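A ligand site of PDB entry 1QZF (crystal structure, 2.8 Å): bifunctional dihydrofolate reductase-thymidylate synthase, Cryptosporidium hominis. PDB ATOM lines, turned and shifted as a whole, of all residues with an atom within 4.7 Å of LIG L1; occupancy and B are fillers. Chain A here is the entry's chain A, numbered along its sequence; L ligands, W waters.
O4 of LIG L1 lies close to O of Ile 75 (3.4 Å).
O of Arg 92 sits close to N4 of LIG L1 (3.4 Å).
Residues that only touch LIG L1: Val 10, Gly 20, Ile 21, Leu 25, Gly 55, Cys 113, Gly 114, Gly 115, Ile 118, Tyr 119, Asp 121 and Thr 145.
The nearest printed residue that does not touch LIG L1 is Ser 61 (4.1 Å).
A nitrogen (N5) of LG2 L2 sits close to an oxygen (O14) of LIG L1.
O12 of LIG L1 lies within hydrogen-bond range of N of Gln 24 (3.4 Å).
OG1 of Thr 58 is in hydrogen-bond range of O2 of LIG L1 (2.7 Å).
O14 of LIG L1 is in hydrogen-bond range of N of Ala 11.
N of Ser 117 lies within hydrogen-bond range of O8 of LIG L1, at 3.2 Å.
OG of Ser 78 sits at hydrogen-bond distance from O15 of LIG L1.
A nitrogen (N7) of LIG L1 sits close to the backbone carbonyl oxygen (O) of Ile 19, at 3.1 Å.
O16 of LIG L1 sits at hydrogen-bond distance from OG of Ser 77.
The backbone NH (N) of Lys 57 is in hydrogen-bond range of an oxygen (O3) of LIG L1 (3.3 Å).
O of Gln 24 lies close to O13 of LIG L1, 3.4 Å away.
The backbone NH (N) of Arg 56 lies within hydrogen-bond range of an oxygen (O4) of LIG L1, at 3.0 Å.
N of Gly 23 sits close to O12 of LIG L1 (3.4 Å).
The backbone NH (N) of Thr 58 sits at hydrogen-bond distance from an oxygen (O2) of LIG L1, 3.0 Å away.
The backbone carbonyl oxygen (O) of Val 10 lies within hydrogen-bond range of a nitrogen (N2) of LG2 L2 (3.4 Å).
N of Glu 116 sits at hydrogen-bond distance from O8 of LIG L1 (3.0 Å).
O of Ala 11 sits at hydrogen-bond distance from N7 of LIG L1 (2.6 Å).
OG of Ser 76 is in hydrogen-bond range of O15 of LIG L1 (2.4 Å).
The backbone carbonyl oxygen (O) of Val 9 lies close to a nitrogen (N5) of LG2 L2 (3.3 Å).
An oxygen (O15) of LIG L1 lies within salt-bridge range of the guanidinium group (NH1) of Arg 56, 2.7 Å away.
An oxygen (O1) of LIG L1 lies within hydrogen-bond range of the side-chain hydroxyl (OG) of Ser 117 (2.5 Å).
The backbone NH (N) of Ser 77 is in hydrogen-bond range of an oxygen (O16) of LIG L1, at 2.7 Å.
The backbone carbonyl oxygen (O) of Gly 23 lies within hydrogen-bond range of the side-chain hydroxyl (OG) of Ser 61 (3.2 Å).
The backbone NH (N) of Arg 56 is in hydrogen-bond range of the backbone carbonyl oxygen (O) of Ile 75 (3.3 Å).
The backbone NH of Gly 55 lies within hydrogen-bond range of the backbone carbonyl oxygen of Gly 114, at 3.2 Å.
The side-chain hydroxyl (OG) of Ser 76 sits at hydrogen-bond distance from the backbone NH (N) of Ser 78 (3.3 Å).
The backbone carbonyl oxygen (O) of Lys 57 lies within hydrogen-bond range of the side-chain hydroxyl (OG) of Ser 61 (3.0 Å).
The backbone carbonyl oxygen of Val 9 lies within hydrogen-bond range of the side-chain hydroxyl of Tyr 119, 2.7 Å away.
The backbone NH (N) of Thr 145 sits at hydrogen-bond distance from the backbone carbonyl oxygen (O) of Gly 20 (3.1 Å).
The guanidinium group of Arg 92 sits close to the backbone carbonyl oxygen of Ser 78, 3.4 Å away.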
ATOM      1  N   VAL A   9     -11.407  28.394  19.524  1.00  0.00           N
ATOM      2  CA  VAL A   9     -12.757  28.808  19.794  1.00  0.00           C
ATOM      3  C   VAL A   9     -13.348  27.639  20.531  1.00  0.00           C
ATOM      4  O   VAL A   9     -13.378  26.535  20.013  1.00  0.00           O
ATOM      5  CB  VAL A   9     -13.560  29.019  18.531  1.00  0.00           C
ATOM      6  CG1 VAL A   9     -14.928  29.561  18.883  1.00  0.00           C
ATOM      7  CG2 VAL A   9     -12.834  29.987  17.623  1.00  0.00           C
ATOM      8  N   VAL A  10     -13.806  27.871  21.756  1.00  0.00           N
ATOM      9  CA  VAL A  10     -14.367  26.786  22.524  1.00  0.00           C
ATOM     10  C   VAL A  10     -15.381  27.299  23.537  1.00  0.00           C
ATOM     11  O   VAL A  10     -15.381  28.468  23.917  1.00  0.00           O
ATOM     12  CB  VAL A  10     -13.258  25.997  23.253  1.00  0.00           C
ATOM     13  CG1 VAL A  10     -12.488  26.925  24.175  1.00  0.00           C
ATOM     14  CG2 VAL A  10     -13.832  24.823  24.024  1.00  0.00           C
ATOM     15  N   ALA A  11     -16.249  26.388  23.948  1.00  0.00           N
ATOM     16  CA  ALA A  11     -17.272  26.672  24.931  1.00  0.00           C
ATOM     17  C   ALA A  11     -17.165  25.569  25.980  1.00  0.00           C
ATOM     18  O   ALA A  11     -17.377  24.401  25.661  1.00  0.00           O
ATOM     19  CB  ALA A  11     -18.631  26.666  24.273  1.00  0.00           C
ATOM     20  N   ILE A  19     -16.749  20.287  27.877  1.00  0.00           N
ATOM     21  CA  ILE A  19     -17.143  20.706  26.540  1.00  0.00           C
ATOM     22  C   ILE A  19     -17.912  19.656  25.739  1.00  0.00           C
ATOM     23  O   ILE A  19     -18.518  19.980  24.719  1.00  0.00           O
ATOM     24  CB  ILE A  19     -15.927  21.132  25.700  1.00  0.00           C
ATOM     25  CG1 ILE A  19     -15.054  19.919  25.403  1.00  0.00           C
ATOM     26  CG2 ILE A  19     -15.130  22.184  26.445  1.00  0.00           C
ATOM     27  CD1 ILE A  19     -14.020  20.173  24.352  1.00  0.00           C
ATOM     28  N   GLY A  20     -17.886  18.408  26.177  1.00  0.00           N
ATOM     29  CA  GLY A  20     -18.583  17.385  25.431  1.00  0.00           C
ATOM     30  C   GLY A  20     -19.104  16.207  26.231  1.00  0.00           C
ATOM     31  O   GLY A  20     -18.646  15.914  27.338  1.00  0.00           O
ATOM     32  N   ILE A  21     -20.086  15.529  25.641  1.00  0.00           N
ATOM     33  CA  ILE A  21     -20.705  14.365  26.251  1.00  0.00           C
ATOM     34  C   ILE A  21     -21.274  13.515  25.122  1.00  0.00           C
ATOM     35  O   ILE A  21     -22.124  13.959  24.359  1.00  0.00           O
ATOM     36  CB  ILE A  21     -21.830  14.794  27.237  1.00  0.00           C
ATOM     37  CG1 ILE A  21     -22.479  13.554  27.846  1.00  0.00           C
ATOM     38  CG2 ILE A  21     -22.831  15.699  26.536  1.00  0.00           C
ATOM     39  CD1 ILE A  21     -21.544  12.723  28.653  1.00  0.00           C
ATOM     40  N   ASN A  22     -20.755  12.286  25.004  1.00  0.00           N
ATOM     41  CA  ASN A  22     -21.186  11.355  23.972  1.00  0.00           C
ATOM     42  C   ASN A  22     -21.251  12.029  22.609  1.00  0.00           C
ATOM     43  O   ASN A  22     -22.285  11.983  21.942  1.00  0.00           O
ATOM     44  CB  ASN A  22     -22.553  10.776  24.292  1.00  0.00           C
ATOM     45  CG  ASN A  22     -22.628  10.201  25.689  1.00  0.00           C
ATOM     46  OD1 ASN A  22     -21.846   9.314  26.055  1.00  0.00           O
ATOM     47  ND2 ASN A  22     -23.584  10.693  26.480  1.00  0.00           N
ATOM     48  N   GLY A  23     -20.162  12.663  22.208  1.00  0.00           N
ATOM     49  CA  GLY A  23     -20.121  13.328  20.905  1.00  0.00           C
ATOM     50  C   GLY A  23     -21.074  14.486  20.706  1.00  0.00           C
ATOM     51  O   GLY A  23     -21.335  14.900  19.585  1.00  0.00           O
ATOM     52  N   GLN A  24     -21.592  15.034  21.798  1.00  0.00           N
ATOM     53  CA  GLN A  24     -22.513  16.155  21.676  1.00  0.00           C
ATOM     54  C   GLN A  24     -22.114  17.299  22.584  1.00  0.00           C
ATOM     55  O   GLN A  24     -21.361  17.120  23.544  1.00  0.00           O
ATOM     56  CB  GLN A  24     -23.924  15.702  22.038  1.00  0.00           C
ATOM     57  CG  GLN A  24     -24.579  14.728  21.089  1.00  0.00           C
ATOM     58  CD  GLN A  24     -25.936  14.273  21.595  1.00  0.00           C
ATOM     59  OE1 GLN A  24     -26.721  13.697  20.843  1.00  0.00           O
ATOM     60  NE2 GLN A  24     -26.202  14.508  22.873  1.00  0.00           N
ATOM     61  N   LEU A  25     -22.612  18.488  22.286  1.00  0.00           N
ATOM     62  CA  LEU A  25     -22.338  19.627  23.141  1.00  0.00           C
ATOM     63  C   LEU A  25     -23.255  19.357  24.317  1.00  0.00           C
ATOM     64  O   LEU A  25     -24.384  18.917  24.130  1.00  0.00           O
ATOM     65  CB  LEU A  25     -22.705  20.918  22.443  1.00  0.00           C
ATOM     66  CG  LEU A  25     -21.812  21.241  21.250  1.00  0.00           C
ATOM     67  CD1 LEU A  25     -22.380  22.409  20.477  1.00  0.00           C
ATOM     68  CD2 LEU A  25     -20.410  21.544  21.741  1.00  0.00           C
ATOM     69  N   TRP A  27     -25.059  21.119  25.969  1.00  0.00           N
ATOM     70  CA  TRP A  27     -26.089  22.143  26.114  1.00  0.00           C
ATOM     71  C   TRP A  27     -26.369  22.700  24.733  1.00  0.00           C
ATOM     72  O   TRP A  27     -25.633  22.430  23.808  1.00  0.00           O
ATOM     73  CB  TRP A  27     -25.548  23.261  27.021  1.00  0.00           C
ATOM     74  CG  TRP A  27     -24.271  23.833  26.481  1.00  0.00           C
ATOM     75  CD1 TRP A  27     -24.106  24.529  25.316  1.00  0.00           C
ATOM     76  CD2 TRP A  27     -22.957  23.645  27.014  1.00  0.00           C
ATOM     77  NE1 TRP A  27     -22.779  24.770  25.085  1.00  0.00           N
ATOM     78  CE2 TRP A  27     -22.047  24.240  26.114  1.00  0.00           C
ATOM     79  CE3 TRP A  27     -22.469  23.031  28.171  1.00  0.00           C
ATOM     80  CZ2 TRP A  27     -20.669  24.231  26.327  1.00  0.00           C
ATOM     81  CZ3 TRP A  27     -21.086  23.025  28.376  1.00  0.00           C
ATOM     82  CH2 TRP A  27     -20.211  23.628  27.460  1.00  0.00           C
ATOM     83  N   GLY A  55     -10.667  17.786  15.196  1.00  0.00           N
ATOM     84  CA  GLY A  55     -10.402  16.369  15.290  1.00  0.00           C
ATOM     85  C   GLY A  55     -11.462  15.631  14.501  1.00  0.00           C
ATOM     86  O   GLY A  55     -12.510  16.205  14.212  1.00  0.00           O
ATOM     87  N   ARG A  56     -11.212  14.376  14.148  1.00  0.00           N
ATOM     88  CA  ARG A  56     -12.172  13.599  13.390  1.00  0.00           C
ATOM     89  C   ARG A  56     -13.506  13.463  14.112  1.00  0.00           C
ATOM     90  O   ARG A  56     -14.564  13.620  13.508  1.00  0.00           O
ATOM     91  CB  ARG A  56     -11.660  12.195  13.102  1.00  0.00           C
ATOM     92  CG  ARG A  56     -12.539  11.494  12.102  1.00  0.00           C
ATOM     93  CD  ARG A  56     -12.536  10.006  12.320  1.00  0.00           C
ATOM     94  NE  ARG A  56     -13.429   9.630  13.413  1.00  0.00           N
ATOM     95  CZ  ARG A  56     -13.055   8.902  14.464  1.00  0.00           C
ATOM     96  NH1 ARG A  56     -11.808   8.485  14.568  1.00  0.00           N
ATOM     97  NH2 ARG A  56     -13.932   8.589  15.396  1.00  0.00           N
ATOM     98  N   LYS A  57     -13.451  13.161  15.409  1.00  0.00           N
ATOM     99  CA  LYS A  57     -14.667  13.017  16.186  1.00  0.00           C
ATOM    100  C   LYS A  57     -15.565  14.261  16.083  1.00  0.00           C
ATOM    101  O   LYS A  57     -16.785  14.142  15.946  1.00  0.00           O
ATOM    102  CB  LYS A  57     -14.321  12.705  17.654  1.00  0.00           C
ATOM    103  CG  LYS A  57     -13.905  11.261  17.914  1.00  0.00           C
ATOM    104  CD  LYS A  57     -13.958  10.960  19.409  1.00  0.00           C
ATOM    105  CE  LYS A  57     -13.900   9.451  19.738  1.00  0.00           C
ATOM    106  NZ  LYS A  57     -12.557   8.839  19.589  1.00  0.00           N
ATOM    107  N   THR A  58     -14.979  15.460  16.142  1.00  0.00           N
ATOM    108  CA  THR A  58     -15.766  16.680  16.033  1.00  0.00           C
ATOM    109  C   THR A  58     -16.352  16.751  14.627  1.00  0.00           C
ATOM    110  O   THR A  58     -17.485  17.174  14.433  1.00  0.00           O
ATOM    111  CB  THR A  58     -14.909  17.933  16.316  1.00  0.00           C
ATOM    112  OG1 THR A  58     -14.538  17.947  17.693  1.00  0.00           O
ATOM    113  CG2 THR A  58     -15.690  19.201  16.008  1.00  0.00           C
ATOM    114  N   SER A  61     -19.354  15.000  14.594  1.00  0.00           N
ATOM    115  CA  SER A  61     -20.358  15.791  15.313  1.00  0.00           C
ATOM    116  C   SER A  61     -21.000  16.840  14.418  1.00  0.00           C
ATOM    117  O   SER A  61     -22.200  17.100  14.534  1.00  0.00           O
ATOM    118  CB  SER A  61     -19.708  16.481  16.520  1.00  0.00           C
ATOM    119  OG  SER A  61     -19.097  15.523  17.362  1.00  0.00           O
ATOM    120  N   ILE A  75      -8.217  16.469  11.146  1.00  0.00           N
ATOM    121  CA  ILE A  75      -7.017  15.763  11.543  1.00  0.00           C
ATOM    122  C   ILE A  75      -7.455  14.351  11.841  1.00  0.00           C
ATOM    123  O   ILE A  75      -8.279  14.122  12.729  1.00  0.00           O
ATOM    124  CB  ILE A  75      -6.363  16.368  12.815  1.00  0.00           C
ATOM    125  CG1 ILE A  75      -5.371  17.478  12.441  1.00  0.00           C
ATOM    126  CG2 ILE A  75      -5.598  15.295  13.562  1.00  0.00           C
ATOM    127  CD1 ILE A  75      -5.994  18.685  11.801  1.00  0.00           C
ATOM    128  N   SER A  76      -6.937  13.391  11.092  1.00  0.00           N
ATOM    129  CA  SER A  76      -7.265  11.990  11.311  1.00  0.00           C
ATOM    130  C   SER A  76      -6.236  11.094  10.674  1.00  0.00           C
ATOM    131  O   SER A  76      -5.683  11.412   9.612  1.00  0.00           O
ATOM    132  CB  SER A  76      -8.636  11.648  10.736  1.00  0.00           C
ATOM    133  OG  SER A  76      -8.896  10.272  10.895  1.00  0.00           O
ATOM    134  N   SER A  77      -5.973   9.963  11.318  1.00  0.00           N
ATOM    135  CA  SER A  77      -5.004   8.988  10.833  1.00  0.00           C
ATOM    136  C   SER A  77      -5.618   8.140   9.728  1.00  0.00           C
ATOM    137  O   SER A  77      -4.931   7.773   8.781  1.00  0.00           O
ATOM    138  CB  SER A  77      -4.568   8.087  11.970  1.00  0.00           C
ATOM    139  OG  SER A  77      -5.634   7.213  12.315  1.00  0.00           O
ATOM    140  N   SER A  78      -6.906   7.831   9.865  1.00  0.00           N
ATOM    141  CA  SER A  78      -7.613   6.994   8.908  1.00  0.00           C
ATOM    142  C   SER A  78      -8.294   7.694   7.723  1.00  0.00           C
ATOM    143  O   SER A  78      -8.006   7.397   6.579  1.00  0.00           O
ATOM    144  CB  SER A  78      -8.669   6.166   9.654  1.00  0.00           C
ATOM    145  OG  SER A  78      -9.669   6.986  10.239  1.00  0.00           O
ATOM    146  N   ARG A  92      -2.776  14.142   8.436  1.00  0.00           N
ATOM    147  CA  ARG A  92      -2.427  13.077   9.360  1.00  0.00           C
ATOM    148  C   ARG A  92      -2.045  13.471  10.774  1.00  0.00           C
ATOM    149  O   ARG A  92      -2.200  12.674  11.702  1.00  0.00           O
ATOM    150  CB  ARG A  92      -1.334  12.212   8.749  1.00  0.00           C
ATOM    151  CG  ARG A  92      -1.786  11.510   7.481  1.00  0.00           C
ATOM    152  CD  ARG A  92      -3.074  10.734   7.724  1.00  0.00           C
ATOM    153  NE  ARG A  92      -3.623  10.190   6.480  1.00  0.00           N
ATOM    154  CZ  ARG A  92      -4.873   9.765   6.340  1.00  0.00           C
ATOM    155  NH1 ARG A  92      -5.729   9.805   7.365  1.00  0.00           N
ATOM    156  NH2 ARG A  92      -5.282   9.300   5.178  1.00  0.00           N
ATOM    157  N   ASN A  93      -1.523  14.684  10.950  1.00  0.00           N
ATOM    158  CA  ASN A  93      -1.150  15.160  12.283  1.00  0.00           C
ATOM    159  C   ASN A  93      -1.424  16.651  12.365  1.00  0.00           C
ATOM    160  O   ASN A  93      -1.469  17.342  11.346  1.00  0.00           O
ATOM    161  CB  ASN A  93       0.325  14.862  12.614  1.00  0.00           C
ATOM    162  CG  ASN A  93       1.295  15.812  11.945  1.00  0.00           C
ATOM    163  OD1 ASN A  93       1.522  15.742  10.740  1.00  0.00           O
ATOM    164  ND2 ASN A  93       1.888  16.712  12.723  1.00  0.00           N
ATOM    165  N   CYS A 113     -10.769  24.578  16.025  1.00  0.00           N
ATOM    166  CA  CYS A 113     -12.148  24.380  16.407  1.00  0.00           C
ATOM    167  C   CYS A 113     -12.581  23.188  17.230  1.00  0.00           C
ATOM    168  O   CYS A 113     -13.742  22.813  17.190  1.00  0.00           O
ATOM    169  CB  CYS A 113     -13.020  24.450  15.165  1.00  0.00           C
ATOM    170  SG  CYS A 113     -12.866  25.998  14.282  1.00  0.00           S
ATOM    171  N   GLY A 114     -11.684  22.566  17.968  1.00  0.00           N
ATOM    172  CA  GLY A 114     -12.210  21.491  18.761  1.00  0.00           C
ATOM    173  C   GLY A 114     -11.692  20.085  18.739  1.00  0.00           C
ATOM    174  O   GLY A 114     -11.143  19.587  17.751  1.00  0.00           O
ATOM    175  N   GLY A 115     -11.974  19.451  19.873  1.00  0.00           N
ATOM    176  CA  GLY A 115     -11.572  18.102  20.143  1.00  0.00           C
ATOM    177  C   GLY A 115     -10.649  18.255  21.327  1.00  0.00           C
ATOM    178  O   GLY A 115      -9.586  18.864  21.199  1.00  0.00           O
ATOM    179  N   GLU A 116     -11.047  17.745  22.484  1.00  0.00           N
ATOM    180  CA  GLU A 116     -10.197  17.852  23.653  1.00  0.00           C
ATOM    181  C   GLU A 116      -8.773  17.518  23.227  1.00  0.00           C
ATOM    182  O   GLU A 116      -7.839  18.220  23.600  1.00  0.00           O
ATOM    183  CB  GLU A 116     -10.650  16.877  24.747  1.00  0.00           C
ATOM    184  CG  GLU A 116      -9.664  16.803  25.894  1.00  0.00           C
ATOM    185  CD  GLU A 116     -10.224  16.075  27.081  1.00  0.00           C
ATOM    186  OE1 GLU A 116      -9.458  15.887  28.058  1.00  0.00           O
ATOM    187  OE2 GLU A 116     -11.417  15.703  27.061  1.00  0.00           O
ATOM    188  N   SER A 117      -8.628  16.472  22.428  1.00  0.00           N
ATOM    189  CA  SER A 117      -7.319  16.053  21.957  1.00  0.00           C
ATOM    190  C   SER A 117      -6.662  17.111  21.097  1.00  0.00           C
ATOM    191  O   SER A 117      -5.498  17.446  21.296  1.00  0.00           O
ATOM    192  CB  SER A 117      -7.441  14.746  21.169  1.00  0.00           C
ATOM    193  OG  SER A 117      -8.146  14.950  19.961  1.00  0.00           O
ATOM    194  N   ILE A 118      -7.396  17.641  20.141  1.00  0.00           N
ATOM    195  CA  ILE A 118      -6.844  18.656  19.262  1.00  0.00           C
ATOM    196  C   ILE A 118      -6.544  19.938  20.022  1.00  0.00           C
ATOM    197  O   ILE A 118      -5.550  20.608  19.742  1.00  0.00           O
ATOM    198  CB  ILE A 118      -7.784  18.959  18.095  1.00  0.00           C
ATOM    199  CG1 ILE A 118      -8.015  17.693  17.272  1.00  0.00           C
ATOM    200  CG2 ILE A 118      -7.176  20.034  17.202  1.00  0.00           C
ATOM    201  CD1 ILE A 118      -6.780  17.181  16.578  1.00  0.00           C
ATOM    202  N   TYR A 119      -7.385  20.270  20.985  1.00  0.00           N
ATOM    203  CA  TYR A 119      -7.142  21.473  21.775  1.00  0.00           C
ATOM    204  C   TYR A 119      -5.839  21.280  22.535  1.00  0.00           C
ATOM    205  O   TYR A 119      -4.902  22.068  22.411  1.00  0.00           O
ATOM    206  CB  TYR A 119      -8.276  21.693  22.787  1.00  0.00           C
ATOM    207  CG  TYR A 119      -9.564  22.262  22.214  1.00  0.00           C
ATOM    208  CD1 TYR A 119      -9.533  23.319  21.303  1.00  0.00           C
ATOM    209  CD2 TYR A 119     -10.794  21.795  22.641  1.00  0.00           C
ATOM    210  CE1 TYR A 119     -10.702  23.889  20.839  1.00  0.00           C
ATOM    211  CE2 TYR A 119     -11.968  22.361  22.186  1.00  0.00           C
ATOM    212  CZ  TYR A 119     -11.924  23.411  21.291  1.00  0.00           C
ATOM    213  OH  TYR A 119     -13.094  23.981  20.852  1.00  0.00           O
ATOM    214  N   ASP A 121      -3.347  19.326  22.135  1.00  0.00           N
ATOM    215  CA  ASP A 121      -2.150  19.305  21.310  1.00  0.00           C
ATOM    216  C   ASP A 121      -1.784  20.679  20.789  1.00  0.00           C
ATOM    217  O   ASP A 121      -0.604  21.023  20.727  1.00  0.00           O
ATOM    218  CB  ASP A 121      -2.319  18.357  20.128  1.00  0.00           C
ATOM    219  CG  ASP A 121      -2.008  16.923  20.493  1.00  0.00           C
ATOM    220  OD1 ASP A 121      -2.240  16.045  19.641  1.00  0.00           O
ATOM    221  OD2 ASP A 121      -1.535  16.686  21.621  1.00  0.00           O
ATOM    222  N   ASP A 144     -17.673  14.194  29.284  1.00  0.00           N
ATOM    223  CA  ASP A 144     -16.689  13.161  28.995  1.00  0.00           C
ATOM    224  C   ASP A 144     -15.534  13.772  28.212  1.00  0.00           C
ATOM    225  O   ASP A 144     -14.522  13.123  27.997  1.00  0.00           O
ATOM    226  CB  ASP A 144     -17.286  11.967  28.233  1.00  0.00           C
ATOM    227  CG  ASP A 144     -17.896  12.356  26.904  1.00  0.00           C
ATOM    228  OD1 ASP A 144     -17.358  13.248  26.223  1.00  0.00           O
ATOM    229  OD2 ASP A 144     -18.920  11.737  26.525  1.00  0.00           O
ATOM    230  N   THR A 145     -15.691  15.020  27.809  1.00  0.00           N
ATOM    231  CA  THR A 145     -14.654  15.737  27.089  1.00  0.00           C
ATOM    232  C   THR A 145     -14.402  17.079  27.771  1.00  0.00           C
ATOM    233  O   THR A 145     -15.337  17.761  28.172  1.00  0.00           O
ATOM    234  CB  THR A 145     -15.047  15.987  25.641  1.00  0.00           C
ATOM    235  OG1 THR A 145     -15.318  14.747  25.005  1.00  0.00           O
ATOM    236  CG2 THR A 145     -13.925  16.697  24.907  1.00  0.00           C
HETATM  237  P1  LIG L   1     -11.693  15.246  18.796  1.00  0.00           P
HETATM  238  O1  LIG L   1     -10.348  15.759  19.095  1.00  0.00           O
HETATM  239  O2  LIG L   1     -12.685  15.962  17.955  1.00  0.00           O
HETATM  240  O3  LIG L   1     -11.248  14.148  17.706  1.00  0.00           O
HETATM  241  C1  LIG L   1     -10.328  13.099  18.007  1.00  0.00           C
HETATM  242  C2  LIG L   1      -9.819  12.454  16.718  1.00  0.00           C
HETATM  243  O4  LIG L   1      -8.991  13.358  15.919  1.00  0.00           O
HETATM  244  C3  LIG L   1      -8.958  11.218  16.927  1.00  0.00           C
HETATM  245  O5  LIG L   1      -9.781  10.056  17.067  1.00  0.00           O
HETATM  246  C4  LIG L   1      -8.219  11.134  15.625  1.00  0.00           C
HETATM  247  O6  LIG L   1      -9.078  10.598  14.623  1.00  0.00           O
HETATM  248  C5  LIG L   1      -7.890  12.588  15.292  1.00  0.00           C
HETATM  249  N1  LIG L   1      -6.623  12.949  15.976  1.00  0.00           N
HETATM  250  C6  LIG L   1      -6.492  13.551  17.169  1.00  0.00           C
HETATM  251  N2  LIG L   1      -5.199  13.691  17.447  1.00  0.00           N
HETATM  252  C7  LIG L   1      -4.498  13.174  16.442  1.00  0.00           C
HETATM  253  C8  LIG L   1      -3.141  13.048  16.191  1.00  0.00           C
HETATM  254  N3  LIG L   1      -2.253  13.481  17.079  1.00  0.00           N
HETATM  255  N4  LIG L   1      -2.730  12.471  15.024  1.00  0.00           N
HETATM  256  C9  LIG L   1      -3.619  12.029  14.132  1.00  0.00           C
HETATM  257  N5  LIG L   1      -4.936  12.141  14.362  1.00  0.00           N
HETATM  258  C10 LIG L   1      -5.396  12.707  15.509  1.00  0.00           C
HETATM  259  O7  LIG L   1     -12.346  14.129  19.807  1.00  0.00           O
HETATM  260  P2  LIG L   1     -12.686  14.497  21.374  1.00  0.00           P
HETATM  261  O8  LIG L   1     -11.309  14.886  21.775  1.00  0.00           O
HETATM  262  O9  LIG L   1     -13.339  13.225  21.742  1.00  0.00           O
HETATM  263  O10 LIG L   1     -13.643  15.747  20.927  1.00  0.00           O
HETATM  264  C11 LIG L   1     -15.021  15.551  20.536  1.00  0.00           C
HETATM  265  C12 LIG L   1     -15.959  15.848  21.725  1.00  0.00           C
HETATM  266  O11 LIG L   1     -15.716  17.252  22.105  1.00  0.00           O
HETATM  267  C13 LIG L   1     -17.428  15.814  21.302  1.00  0.00           C
HETATM  268  O12 LIG L   1     -18.252  15.480  22.418  1.00  0.00           O
HETATM  269  C14 LIG L   1     -17.725  17.222  20.872  1.00  0.00           C
HETATM  270  O13 LIG L   1     -19.104  17.525  21.050  1.00  0.00           O
HETATM  271  C15 LIG L   1     -16.916  18.038  21.843  1.00  0.00           C
HETATM  272  N6  LIG L   1     -16.610  19.403  21.370  1.00  0.00           N
HETATM  273  C16 LIG L   1     -16.989  20.512  22.168  1.00  0.00           C
HETATM  274  C17 LIG L   1     -16.616  21.795  21.774  1.00  0.00           C
HETATM  275  C18 LIG L   1     -16.988  23.016  22.639  1.00  0.00           C
HETATM  276  O14 LIG L   1     -16.632  24.145  22.316  1.00  0.00           O
HETATM  277  N7  LIG L   1     -17.701  22.747  23.725  1.00  0.00           N
HETATM  278  C19 LIG L   1     -15.869  21.974  20.593  1.00  0.00           C
HETATM  279  C20 LIG L   1     -15.498  20.885  19.799  1.00  0.00           C
HETATM  280  C21 LIG L   1     -15.866  19.597  20.181  1.00  0.00           C
HETATM  281  P3  LIG L   1      -8.671   9.228  13.888  1.00  0.00           P
HETATM  282  O15 LIG L   1      -9.839   9.034  12.787  1.00  0.00           O
HETATM  283  O16 LIG L   1      -7.290   9.057  13.494  1.00  0.00           O
HETATM  284  O17 LIG L   1      -9.090   8.260  14.917  1.00  0.00           O
HETATM  285  N1  LG2 L   2     -17.004  26.906  20.293  1.00  0.00           N
HETATM  286  C1  LG2 L   2     -18.094  27.596  20.853  1.00  0.00           C
HETATM  287  N2  LG2 L   2     -17.900  28.684  21.588  1.00  0.00           N
HETATM  288  N3  LG2 L   2     -19.385  27.124  20.605  1.00  0.00           N
HETATM  289  C2  LG2 L   2     -19.584  25.988  19.808  1.00  0.00           C
HETATM  290  O1  LG2 L   2     -20.713  25.505  19.715  1.00  0.00           O
HETATM  291  C3  LG2 L   2     -18.506  25.324  19.240  1.00  0.00           C
HETATM  292  N4  LG2 L   2     -18.699  24.158  18.484  1.00  0.00           N
HETATM  293  C4  LG2 L   2     -17.615  23.384  18.033  1.00  0.00           C
HETATM  294  C5  LG2 L   2     -16.318  23.836  18.326  1.00  0.00           C
HETATM  295  N5  LG2 L   2     -16.123  25.021  19.041  1.00  0.00           N
HETATM  296  C6  LG2 L   2     -17.217  25.778  19.504  1.00  0.00           C
HETATM  297  C7  LG2 L   2     -17.739  22.366  17.097  1.00  0.00           C
HETATM  298  N6  LG2 L   2     -18.795  22.003  16.402  1.00  0.00           N
HETATM  299  C8  LG2 L   2     -21.730  24.005  14.599  1.00  0.00           C
HETATM  300  C9  LG2 L   2     -20.855  24.710  15.424  1.00  0.00           C
HETATM  301  C10 LG2 L   2     -19.991  24.021  16.263  1.00  0.00           C
HETATM  302  C11 LG2 L   2     -19.970  22.624  16.282  1.00  0.00           C
HETATM  303  C12 LG2 L   2     -20.890  21.929  15.509  1.00  0.00           C
HETATM  304  C13 LG2 L   2     -21.763  22.621  14.666  1.00  0.00           C
HETATM  305  C14 LG2 L   2     -22.451  24.728  13.462  1.00  0.00           C
HETATM  306  O2  LG2 L   2     -23.400  24.190  12.878  1.00  0.00           O
HETATM  307  N7  LG2 L   2     -22.007  25.941  13.142  1.00  0.00           N
HETATM  308  C15 LG2 L   2     -22.578  26.732  12.037  1.00  0.00           C
HETATM  309  C16 LG2 L   2     -23.977  27.278  12.336  1.00  0.00           C
HETATM  310  C17 LG2 L   2     -24.009  28.244  13.517  1.00  0.00           C
HETATM  311  C18 LG2 L   2     -25.396  28.876  13.649  1.00  0.00           C
HETATM  312  O3  LG2 L   2     -26.198  28.362  14.462  1.00  0.00           O
HETATM  313  O4  LG2 L   2     -25.632  29.868  12.922  1.00  0.00           O
HETATM  314  C19 LG2 L   2     -21.625  27.866  11.639  1.00  0.00           C
HETATM  315  O5  LG2 L   2     -22.085  28.726  10.856  1.00  0.00           O
HETATM  316  O6  LG2 L   2     -20.469  27.834  12.108  1.00  0.00           O
HETATM  317  O   HOH W   1     -15.943  11.595  21.752  1.00  0.00           O
